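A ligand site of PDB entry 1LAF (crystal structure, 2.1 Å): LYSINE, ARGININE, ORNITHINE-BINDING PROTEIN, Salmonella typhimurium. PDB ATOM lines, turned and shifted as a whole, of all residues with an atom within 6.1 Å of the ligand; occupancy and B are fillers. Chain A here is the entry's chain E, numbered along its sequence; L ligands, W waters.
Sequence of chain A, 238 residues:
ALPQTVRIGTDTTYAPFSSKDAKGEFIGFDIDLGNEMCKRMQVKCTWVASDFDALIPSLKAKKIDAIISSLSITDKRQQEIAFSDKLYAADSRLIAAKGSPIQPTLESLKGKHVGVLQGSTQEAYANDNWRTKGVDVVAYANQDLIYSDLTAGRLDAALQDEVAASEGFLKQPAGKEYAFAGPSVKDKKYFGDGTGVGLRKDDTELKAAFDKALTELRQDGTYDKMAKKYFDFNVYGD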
ATOM      1  N   THR A  10      13.126 -27.841 -25.173  1.00  0.00           N
ATOM      2  CA  THR A  10      13.455 -28.186 -23.823  1.00  0.00           C
ATOM      3  C   THR A  10      14.300 -29.458 -23.884  1.00  0.00           C
ATOM      4  O   THR A  10      14.349 -30.184 -24.880  1.00  0.00           O
ATOM      5  CB  THR A  10      12.107 -28.380 -23.024  1.00  0.00           C
ATOM      6  OG1 THR A  10      12.477 -28.389 -21.628  1.00  0.00           O
ATOM      7  CG2 THR A  10      11.320 -29.627 -23.374  1.00  0.00           C
ATOM      8  N   ASP A  11      15.036 -29.724 -22.819  1.00  0.00           N
ATOM      9  CA  ASP A  11      15.841 -30.901 -22.641  1.00  0.00           C
ATOM     10  C   ASP A  11      15.152 -31.641 -21.512  1.00  0.00           C
ATOM     11  O   ASP A  11      15.192 -31.232 -20.336  1.00  0.00           O
ATOM     12  CB  ASP A  11      17.262 -30.464 -22.271  1.00  0.00           C
ATOM     13  CG  ASP A  11      18.007 -31.643 -21.628  1.00  0.00           C
ATOM     14  OD1 ASP A  11      18.158 -32.680 -22.243  1.00  0.00           O
ATOM     15  OD2 ASP A  11      18.368 -31.558 -20.478  1.00  0.00           O
ATOM     16  N   THR A  12      14.623 -32.808 -21.848  1.00  0.00           N
ATOM     17  CA  THR A  12      13.841 -33.554 -20.887  1.00  0.00           C
ATOM     18  C   THR A  12      14.625 -34.459 -19.964  1.00  0.00           C
ATOM     19  O   THR A  12      14.184 -35.585 -19.706  1.00  0.00           O
ATOM     20  CB  THR A  12      12.775 -34.308 -21.708  1.00  0.00           C
ATOM     21  OG1 THR A  12      13.413 -35.061 -22.736  1.00  0.00           O
ATOM     22  CG2 THR A  12      11.856 -33.331 -22.379  1.00  0.00           C
ATOM     23  N   THR A  13      15.805 -34.073 -19.468  1.00  0.00           N
ATOM     24  CA  THR A  13      16.526 -34.903 -18.524  1.00  0.00           C
ATOM     25  C   THR A  13      16.811 -34.046 -17.301  1.00  0.00           C
ATOM     26  O   THR A  13      17.903 -34.062 -16.754  1.00  0.00           O
ATOM     27  CB  THR A  13      17.851 -35.458 -19.163  1.00  0.00           C
ATOM     28  OG1 THR A  13      18.659 -34.364 -19.525  1.00  0.00           O
ATOM     29  CG2 THR A  13      17.638 -36.151 -20.467  1.00  0.00           C
ATOM     30  N   TYR A  14      15.865 -33.236 -16.841  1.00  0.00           N
ATOM     31  CA  TYR A  14      16.096 -32.375 -15.714  1.00  0.00           C
ATOM     32  C   TYR A  14      14.852 -32.282 -14.846  1.00  0.00           C
ATOM     33  O   TYR A  14      14.213 -31.232 -14.635  1.00  0.00           O
ATOM     34  CB  TYR A  14      16.507 -31.001 -16.238  1.00  0.00           C
ATOM     35  CG  TYR A  14      17.665 -30.352 -15.525  1.00  0.00           C
ATOM     36  CD1 TYR A  14      18.921 -30.930 -15.534  1.00  0.00           C
ATOM     37  CD2 TYR A  14      17.437 -29.137 -14.909  1.00  0.00           C
ATOM     38  CE1 TYR A  14      19.975 -30.289 -14.899  1.00  0.00           C
ATOM     39  CE2 TYR A  14      18.493 -28.510 -14.271  1.00  0.00           C
ATOM     40  CZ  TYR A  14      19.754 -29.079 -14.279  1.00  0.00           C
ATOM     41  OH  TYR A  14      20.771 -28.395 -13.650  1.00  0.00           O
ATOM     42  N   SER A  18      11.754 -30.700 -16.295  1.00  0.00           N
ATOM     43  CA  SER A  18      11.500 -31.192 -17.625  1.00  0.00           C
ATOM     44  C   SER A  18      11.915 -32.651 -17.740  1.00  0.00           C
ATOM     45  O   SER A  18      13.103 -32.942 -17.638  1.00  0.00           O
ATOM     46  CB  SER A  18      12.276 -30.303 -18.596  1.00  0.00           C
ATOM     47  OG  SER A  18      11.857 -30.608 -19.913  1.00  0.00           O
ATOM     48  N   ASP A  30       8.422 -26.879 -15.912  1.00  0.00           N
ATOM     49  CA  ASP A  30       8.614 -26.069 -17.110  1.00  0.00           C
ATOM     50  C   ASP A  30       7.553 -26.280 -18.162  1.00  0.00           C
ATOM     51  O   ASP A  30       7.136 -25.332 -18.850  1.00  0.00           O
ATOM     52  CB  ASP A  30       9.927 -26.329 -17.805  1.00  0.00           C
ATOM     53  CG  ASP A  30      11.122 -25.658 -17.179  1.00  0.00           C
ATOM     54  OD1 ASP A  30      10.969 -24.898 -16.242  1.00  0.00           O
ATOM     55  OD2 ASP A  30      12.217 -25.914 -17.632  1.00  0.00           O
ATOM     56  N   PHE A  52      20.644 -30.097 -24.104  1.00  0.00           N
ATOM     57  CA  PHE A  52      20.693 -28.737 -23.554  1.00  0.00           C
ATOM     58  C   PHE A  52      21.599 -27.797 -24.385  1.00  0.00           C
ATOM     59  O   PHE A  52      21.221 -26.678 -24.696  1.00  0.00           O
ATOM     60  CB  PHE A  52      21.182 -28.773 -22.113  1.00  0.00           C
ATOM     61  CG  PHE A  52      21.071 -27.416 -21.426  1.00  0.00           C
ATOM     62  CD1 PHE A  52      19.819 -26.879 -21.133  1.00  0.00           C
ATOM     63  CD2 PHE A  52      22.212 -26.680 -21.167  1.00  0.00           C
ATOM     64  CE1 PHE A  52      19.731 -25.619 -20.588  1.00  0.00           C
ATOM     65  CE2 PHE A  52      22.102 -25.421 -20.612  1.00  0.00           C
ATOM     66  CZ  PHE A  52      20.867 -24.891 -20.330  1.00  0.00           C
ATOM     67  N   LEU A  55      20.084 -26.155 -27.521  1.00  0.00           N
ATOM     68  CA  LEU A  55      18.914 -25.299 -27.465  1.00  0.00           C
ATOM     69  C   LEU A  55      19.141 -23.885 -27.993  1.00  0.00           C
ATOM     70  O   LEU A  55      18.460 -23.442 -28.949  1.00  0.00           O
ATOM     71  CB  LEU A  55      18.408 -25.292 -25.983  1.00  0.00           C
ATOM     72  CG  LEU A  55      17.806 -26.623 -25.410  1.00  0.00           C
ATOM     73  CD1 LEU A  55      17.447 -26.483 -23.944  1.00  0.00           C
ATOM     74  CD2 LEU A  55      16.508 -26.948 -26.110  1.00  0.00           C
ATOM     75  N   SER A  69      13.647 -24.352 -20.383  1.00  0.00           N
ATOM     76  CA  SER A  69      14.436 -25.489 -19.933  1.00  0.00           C
ATOM     77  C   SER A  69      15.329 -25.128 -18.745  1.00  0.00           C
ATOM     78  O   SER A  69      16.535 -25.446 -18.771  1.00  0.00           O
ATOM     79  CB  SER A  69      15.242 -25.943 -21.200  1.00  0.00           C
ATOM     80  OG  SER A  69      15.796 -27.252 -21.231  1.00  0.00           O
ATOM     81  N   SER A  70      14.814 -24.461 -17.674  1.00  0.00           N
ATOM     82  CA  SER A  70      15.671 -23.994 -16.570  1.00  0.00           C
ATOM     83  C   SER A  70      16.870 -23.172 -17.100  1.00  0.00           C
ATOM     84  O   SER A  70      17.980 -23.221 -16.549  1.00  0.00           O
ATOM     85  CB  SER A  70      16.187 -25.184 -15.800  1.00  0.00           C
ATOM     86  OG  SER A  70      15.184 -25.817 -15.033  1.00  0.00           O
ATOM     87  N   LEU A  71      16.585 -22.337 -18.109  1.00  0.00           N
ATOM     88  CA  LEU A  71      17.641 -21.553 -18.751  1.00  0.00           C
ATOM     89  C   LEU A  71      17.906 -20.338 -17.898  1.00  0.00           C
ATOM     90  O   LEU A  71      17.076 -19.452 -17.851  1.00  0.00           O
ATOM     91  CB  LEU A  71      17.191 -21.126 -20.130  1.00  0.00           C
ATOM     92  CG  LEU A  71      18.294 -20.637 -21.054  1.00  0.00           C
ATOM     93  CD1 LEU A  71      19.211 -21.804 -21.345  1.00  0.00           C
ATOM     94  CD2 LEU A  71      17.713 -20.006 -22.315  1.00  0.00           C
ATOM     95  N   SER A  72      18.974 -20.305 -17.156  1.00  0.00           N
ATOM     96  CA  SER A  72      19.267 -19.161 -16.311  1.00  0.00           C
ATOM     97  C   SER A  72      19.562 -17.924 -17.134  1.00  0.00           C
ATOM     98  O   SER A  72      20.132 -18.049 -18.235  1.00  0.00           O
ATOM     99  CB  SER A  72      20.455 -19.482 -15.448  1.00  0.00           C
ATOM    100  OG  SER A  72      20.217 -20.640 -14.646  1.00  0.00           O
ATOM    101  N   ILE A  73      19.121 -16.771 -16.614  1.00  0.00           N
ATOM    102  CA  ILE A  73      19.270 -15.480 -17.287  1.00  0.00           C
ATOM    103  C   ILE A  73      20.653 -14.959 -16.843  1.00  0.00           C
ATOM    104  O   ILE A  73      20.830 -14.634 -15.662  1.00  0.00           O
ATOM    105  CB  ILE A  73      18.169 -14.455 -16.858  1.00  0.00           C
ATOM    106  CG1 ILE A  73      16.821 -15.042 -17.139  1.00  0.00           C
ATOM    107  CG2 ILE A  73      18.287 -13.138 -17.675  1.00  0.00           C
ATOM    108  CD1 ILE A  73      15.714 -14.339 -16.388  1.00  0.00           C
ATOM    109  N   ARG A  77      24.570 -14.782 -21.738  1.00  0.00           N
ATOM    110  CA  ARG A  77      23.482 -15.188 -22.627  1.00  0.00           C
ATOM    111  C   ARG A  77      22.711 -13.992 -23.181  1.00  0.00           C
ATOM    112  O   ARG A  77      22.287 -14.017 -24.344  1.00  0.00           O
ATOM    113  CB  ARG A  77      22.582 -16.144 -21.838  1.00  0.00           C
ATOM    114  CG  ARG A  77      23.238 -17.525 -21.841  1.00  0.00           C
ATOM    115  CD  ARG A  77      22.411 -18.440 -20.997  1.00  0.00           C
ATOM    116  NE  ARG A  77      23.033 -19.749 -20.983  1.00  0.00           N
ATOM    117  CZ  ARG A  77      22.713 -20.690 -20.081  1.00  0.00           C
ATOM    118  NH1 ARG A  77      21.789 -20.447 -19.141  1.00  0.00           N
ATOM    119  NH2 ARG A  77      23.365 -21.863 -20.076  1.00  0.00           N
ATOM    120  N   ALA A  90      17.135 -20.299  -9.340  1.00  0.00           N
ATOM    121  CA  ALA A  90      17.881 -21.468  -9.575  1.00  0.00           C
ATOM    122  C   ALA A  90      19.284 -21.306  -9.014  1.00  0.00           C
ATOM    123  O   ALA A  90      20.095 -20.634  -9.659  1.00  0.00           O
ATOM    124  CB  ALA A  90      17.934 -21.726 -11.082  1.00  0.00           C
ATOM    125  N   LEU A 117      26.856 -30.742 -16.772  1.00  0.00           N
ATOM    126  CA  LEU A 117      26.111 -30.751 -18.026  1.00  0.00           C
ATOM    127  C   LEU A 117      26.781 -29.809 -19.036  1.00  0.00           C
ATOM    128  O   LEU A 117      27.036 -28.637 -18.748  1.00  0.00           O
ATOM    129  CB  LEU A 117      24.673 -30.301 -17.736  1.00  0.00           C
ATOM    130  CG  LEU A 117      23.715 -30.150 -18.896  1.00  0.00           C
ATOM    131  CD1 LEU A 117      23.519 -31.501 -19.508  1.00  0.00           C
ATOM    132  CD2 LEU A 117      22.404 -29.534 -18.411  1.00  0.00           C
ATOM    133  N   GLY A 119      27.139 -27.248 -21.828  1.00  0.00           N
ATOM    134  CA  GLY A 119      26.369 -26.113 -22.266  1.00  0.00           C
ATOM    135  C   GLY A 119      25.806 -25.328 -21.096  1.00  0.00           C
ATOM    136  O   GLY A 119      25.216 -24.264 -21.324  1.00  0.00           O
ATOM    137  N   SER A 120      26.009 -25.803 -19.849  1.00  0.00           N
ATOM    138  CA  SER A 120      25.396 -25.149 -18.696  1.00  0.00           C
ATOM    139  C   SER A 120      26.244 -24.069 -18.046  1.00  0.00           C
ATOM    140  O   SER A 120      27.442 -23.957 -18.333  1.00  0.00           O
ATOM    141  CB  SER A 120      25.063 -26.161 -17.650  1.00  0.00           C
ATOM    142  OG  SER A 120      26.219 -26.793 -17.130  1.00  0.00           O
ATOM    143  N   THR A 121      25.646 -23.297 -17.150  1.00  0.00           N
ATOM    144  CA  THR A 121      26.368 -22.293 -16.381  1.00  0.00           C
ATOM    145  C   THR A 121      27.368 -22.979 -15.451  1.00  0.00           C
ATOM    146  O   THR A 121      28.463 -22.495 -15.191  1.00  0.00           O
ATOM    147  CB  THR A 121      25.405 -21.431 -15.542  1.00  0.00           C
ATOM    148  OG1 THR A 121      24.703 -22.379 -14.744  1.00  0.00           O
ATOM    149  CG2 THR A 121      24.421 -20.576 -16.337  1.00  0.00           C
ATOM    150  N   GLN A 122      27.040 -24.214 -15.023  1.00  0.00           N
ATOM    151  CA  GLN A 122      27.876 -24.997 -14.152  1.00  0.00           C
ATOM    152  C   GLN A 122      29.109 -25.439 -14.926  1.00  0.00           C
ATOM    153  O   GLN A 122      30.189 -25.375 -14.348  1.00  0.00           O
ATOM    154  CB  GLN A 122      27.100 -26.230 -13.656  1.00  0.00           C
ATOM    155  CG  GLN A 122      26.000 -25.973 -12.618  1.00  0.00           C
ATOM    156  CD  GLN A 122      24.650 -25.574 -13.188  1.00  0.00           C
ATOM    157  OE1 GLN A 122      24.407 -25.722 -14.385  1.00  0.00           O
ATOM    158  NE2 GLN A 122      23.697 -25.092 -12.429  1.00  0.00           N
ATOM    159  N   GLN A 143      21.898 -34.678 -18.103  1.00  0.00           N
ATOM    160  CA  GLN A 143      22.015 -34.841 -16.661  1.00  0.00           C
ATOM    161  C   GLN A 143      21.807 -36.271 -16.155  1.00  0.00           C
ATOM    162  O   GLN A 143      22.392 -36.679 -15.134  1.00  0.00           O
ATOM    163  CB  GLN A 143      21.021 -33.892 -15.986  1.00  0.00           C
ATOM    164  CG  GLN A 143      21.108 -33.810 -14.486  1.00  0.00           C
ATOM    165  CD  GLN A 143      22.429 -33.273 -13.964  1.00  0.00           C
ATOM    166  OE1 GLN A 143      22.887 -33.583 -12.871  1.00  0.00           O
ATOM    167  NE2 GLN A 143      23.134 -32.415 -14.677  1.00  0.00           N
ATOM    168  N   ASP A 161      21.784 -27.525 -10.992  1.00  0.00           N
ATOM    169  CA  ASP A 161      20.843 -26.735 -10.191  1.00  0.00           C
ATOM    170  C   ASP A 161      20.381 -27.526  -8.955  1.00  0.00           C
ATOM    171  O   ASP A 161      20.153 -28.748  -8.979  1.00  0.00           O
ATOM    172  CB  ASP A 161      19.612 -26.333 -11.056  1.00  0.00           C
ATOM    173  CG  ASP A 161      19.850 -25.296 -12.144  1.00  0.00           C
ATOM    174  OD1 ASP A 161      20.908 -24.657 -12.191  1.00  0.00           O
ATOM    175  OD2 ASP A 161      18.931 -25.118 -12.946  1.00  0.00           O
ATOM    176  N   THR A 195      15.624 -18.159 -13.903  1.00  0.00           N
ATOM    177  CA  THR A 195      15.538 -18.749 -15.244  1.00  0.00           C
ATOM    178  C   THR A 195      14.426 -18.028 -16.010  1.00  0.00           C
ATOM    179  O   THR A 195      13.553 -17.429 -15.345  1.00  0.00           O
ATOM    180  CB  THR A 195      15.216 -20.264 -15.125  1.00  0.00           C
ATOM    181  OG1 THR A 195      13.911 -20.400 -14.581  1.00  0.00           O
ATOM    182  CG2 THR A 195      16.265 -20.991 -14.279  1.00  0.00           C
HETATM  183  N1  LIG L   1      20.414 -23.676 -15.131  1.00  0.00           N
HETATM  184  C1  LIG L   1      21.528 -24.275 -15.795  1.00  0.00           C
HETATM  185  C2  LIG L   1      21.770 -23.401 -17.040  1.00  0.00           C
HETATM  186  O1  LIG L   1      22.770 -23.604 -17.719  1.00  0.00           O
HETATM  187  C3  LIG L   1      21.178 -25.717 -16.148  1.00  0.00           C
HETATM  188  C4  LIG L   1      19.782 -25.900 -16.738  1.00  0.00           C
HETATM  189  C5  LIG L   1      19.712 -27.251 -17.387  1.00  0.00           C
HETATM  190  N2  LIG L   1      18.370 -27.499 -17.861  1.00  0.00           N
HETATM  191  C6  LIG L   1      18.076 -28.627 -18.516  1.00  0.00           C
HETATM  192  N3  LIG L   1      19.016 -29.497 -18.793  1.00  0.00           N
HETATM  193  N4  LIG L   1      16.853 -28.902 -18.946  1.00  0.00           N
HETATM  194  O2  LIG L   1      20.957 -22.509 -17.320  1.00  0.00           O
HETATM  195  O   HOH W   1      23.217 -28.179 -14.972  1.00  0.00           O
HETATM  196  O   HOH W   2      14.666 -27.896 -17.256  1.00  0.00           O
HETATM  197  O   HOH W   3      20.432 -32.518 -18.759  1.00  0.00           O
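The side-chain carboxylate of Asp 11 is in salt-bridge range of a nitrogen (N3) of the ligand (2.7 Å).
OG of Ser 69 sits at hydrogen-bond distance from N4 of the ligand (3.0 Å).
An oxygen (O2) of the ligand lies within salt-bridge range of the guanidinium group (NH1) of Arg 77, 2.9 Å away.
A nitrogen (N2) of the ligand is in hydrogen-bond range of the backbone carbonyl oxygen (O) of Ser 69.
An oxygen (O1) of the ligand sits at hydrogen-bond distance from the backbone NH (N) of Thr 121 (2.9 Å).
OD2 of Asp 161 is in salt-bridge range of N1 of the ligand (3.0 Å).
A nitrogen (N4) of the ligand lies within hydrogen-bond range of the backbone carbonyl oxygen (O) of Asp 11.
A nitrogen (N1) of the ligand sits at hydrogen-bond distance from the side-chain hydroxyl (OG) of Ser 72 (3.1 Å).
N of Ser 72 is in hydrogen-bond range of O2 of the ligand.
A nitrogen (N1) of the ligand is in hydrogen-bond range of the backbone carbonyl oxygen (O) of Ser 70 (2.9 Å).
The side-chain carboxylate (OD2) of Asp 11 sits at hydrogen-bond distance from the side-chain hydroxyl (OG1) of Thr 13.
N of Ser 69 lies close to OD2 of Asp 30.
OG of Ser 120 lies within hydrogen-bond range of O of Leu 117 (2.6 Å).
The backbone carbonyl oxygen (O) of Gly 119 lies within hydrogen-bond range of the guanidinium group (NH2) of Arg 77 (3.3 Å).
NE2 of Gln 122 is in hydrogen-bond range of OD1 of Asp 161, at 2.8 Å.
The backbone NH (N) of Asp 161 sits at hydrogen-bond distance from the side-chain hydroxyl (OH) of Tyr 14 (3.0 Å).
OE1 of Gln 122 is in hydrogen-bond range of OG1 of Thr 121.
The backbone NH of Asp 11 is in hydrogen-bond range of the side-chain hydroxyl of Ser 69 (3.0 Å).
Merely in contact with the ligand: Ser 120 (3.2 Å), Leu 117 (3.4 Å), Tyr 14 (3.4 Å), Phe 52 (3.5 Å), Gln 122 (3.5 Å) and Leu 71 (3.7 Å).
Of the 24 residues printed, 13 come within 4 Å of the ligand.
Water W2 lies within hydrogen-bond range of a nitrogen (N4) of the ligand (2.9 Å), the side-chain hydroxyl of Ser 70 (3.1 Å), the side-chain carboxylate of Asp 30 (3.2 Å) and the backbone carbonyl oxygen of Ser 69 (3.4 Å).
Water W3 lies within hydrogen-bond range of the side-chain hydroxyl of Thr 13 (2.7 Å), the backbone NH of Gln 143 (2.7 Å), the side-chain carboxylate of Asp 11 (2.9 Å) and a nitrogen (N3) of the ligand (3.3 Å).
Water W1 lies within hydrogen-bond range of the side-chain hydroxyl (OH) of Tyr 14 (2.8 Å) and the side-chain amide oxygen (OE1) of Gln 122 (2.8 Å).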
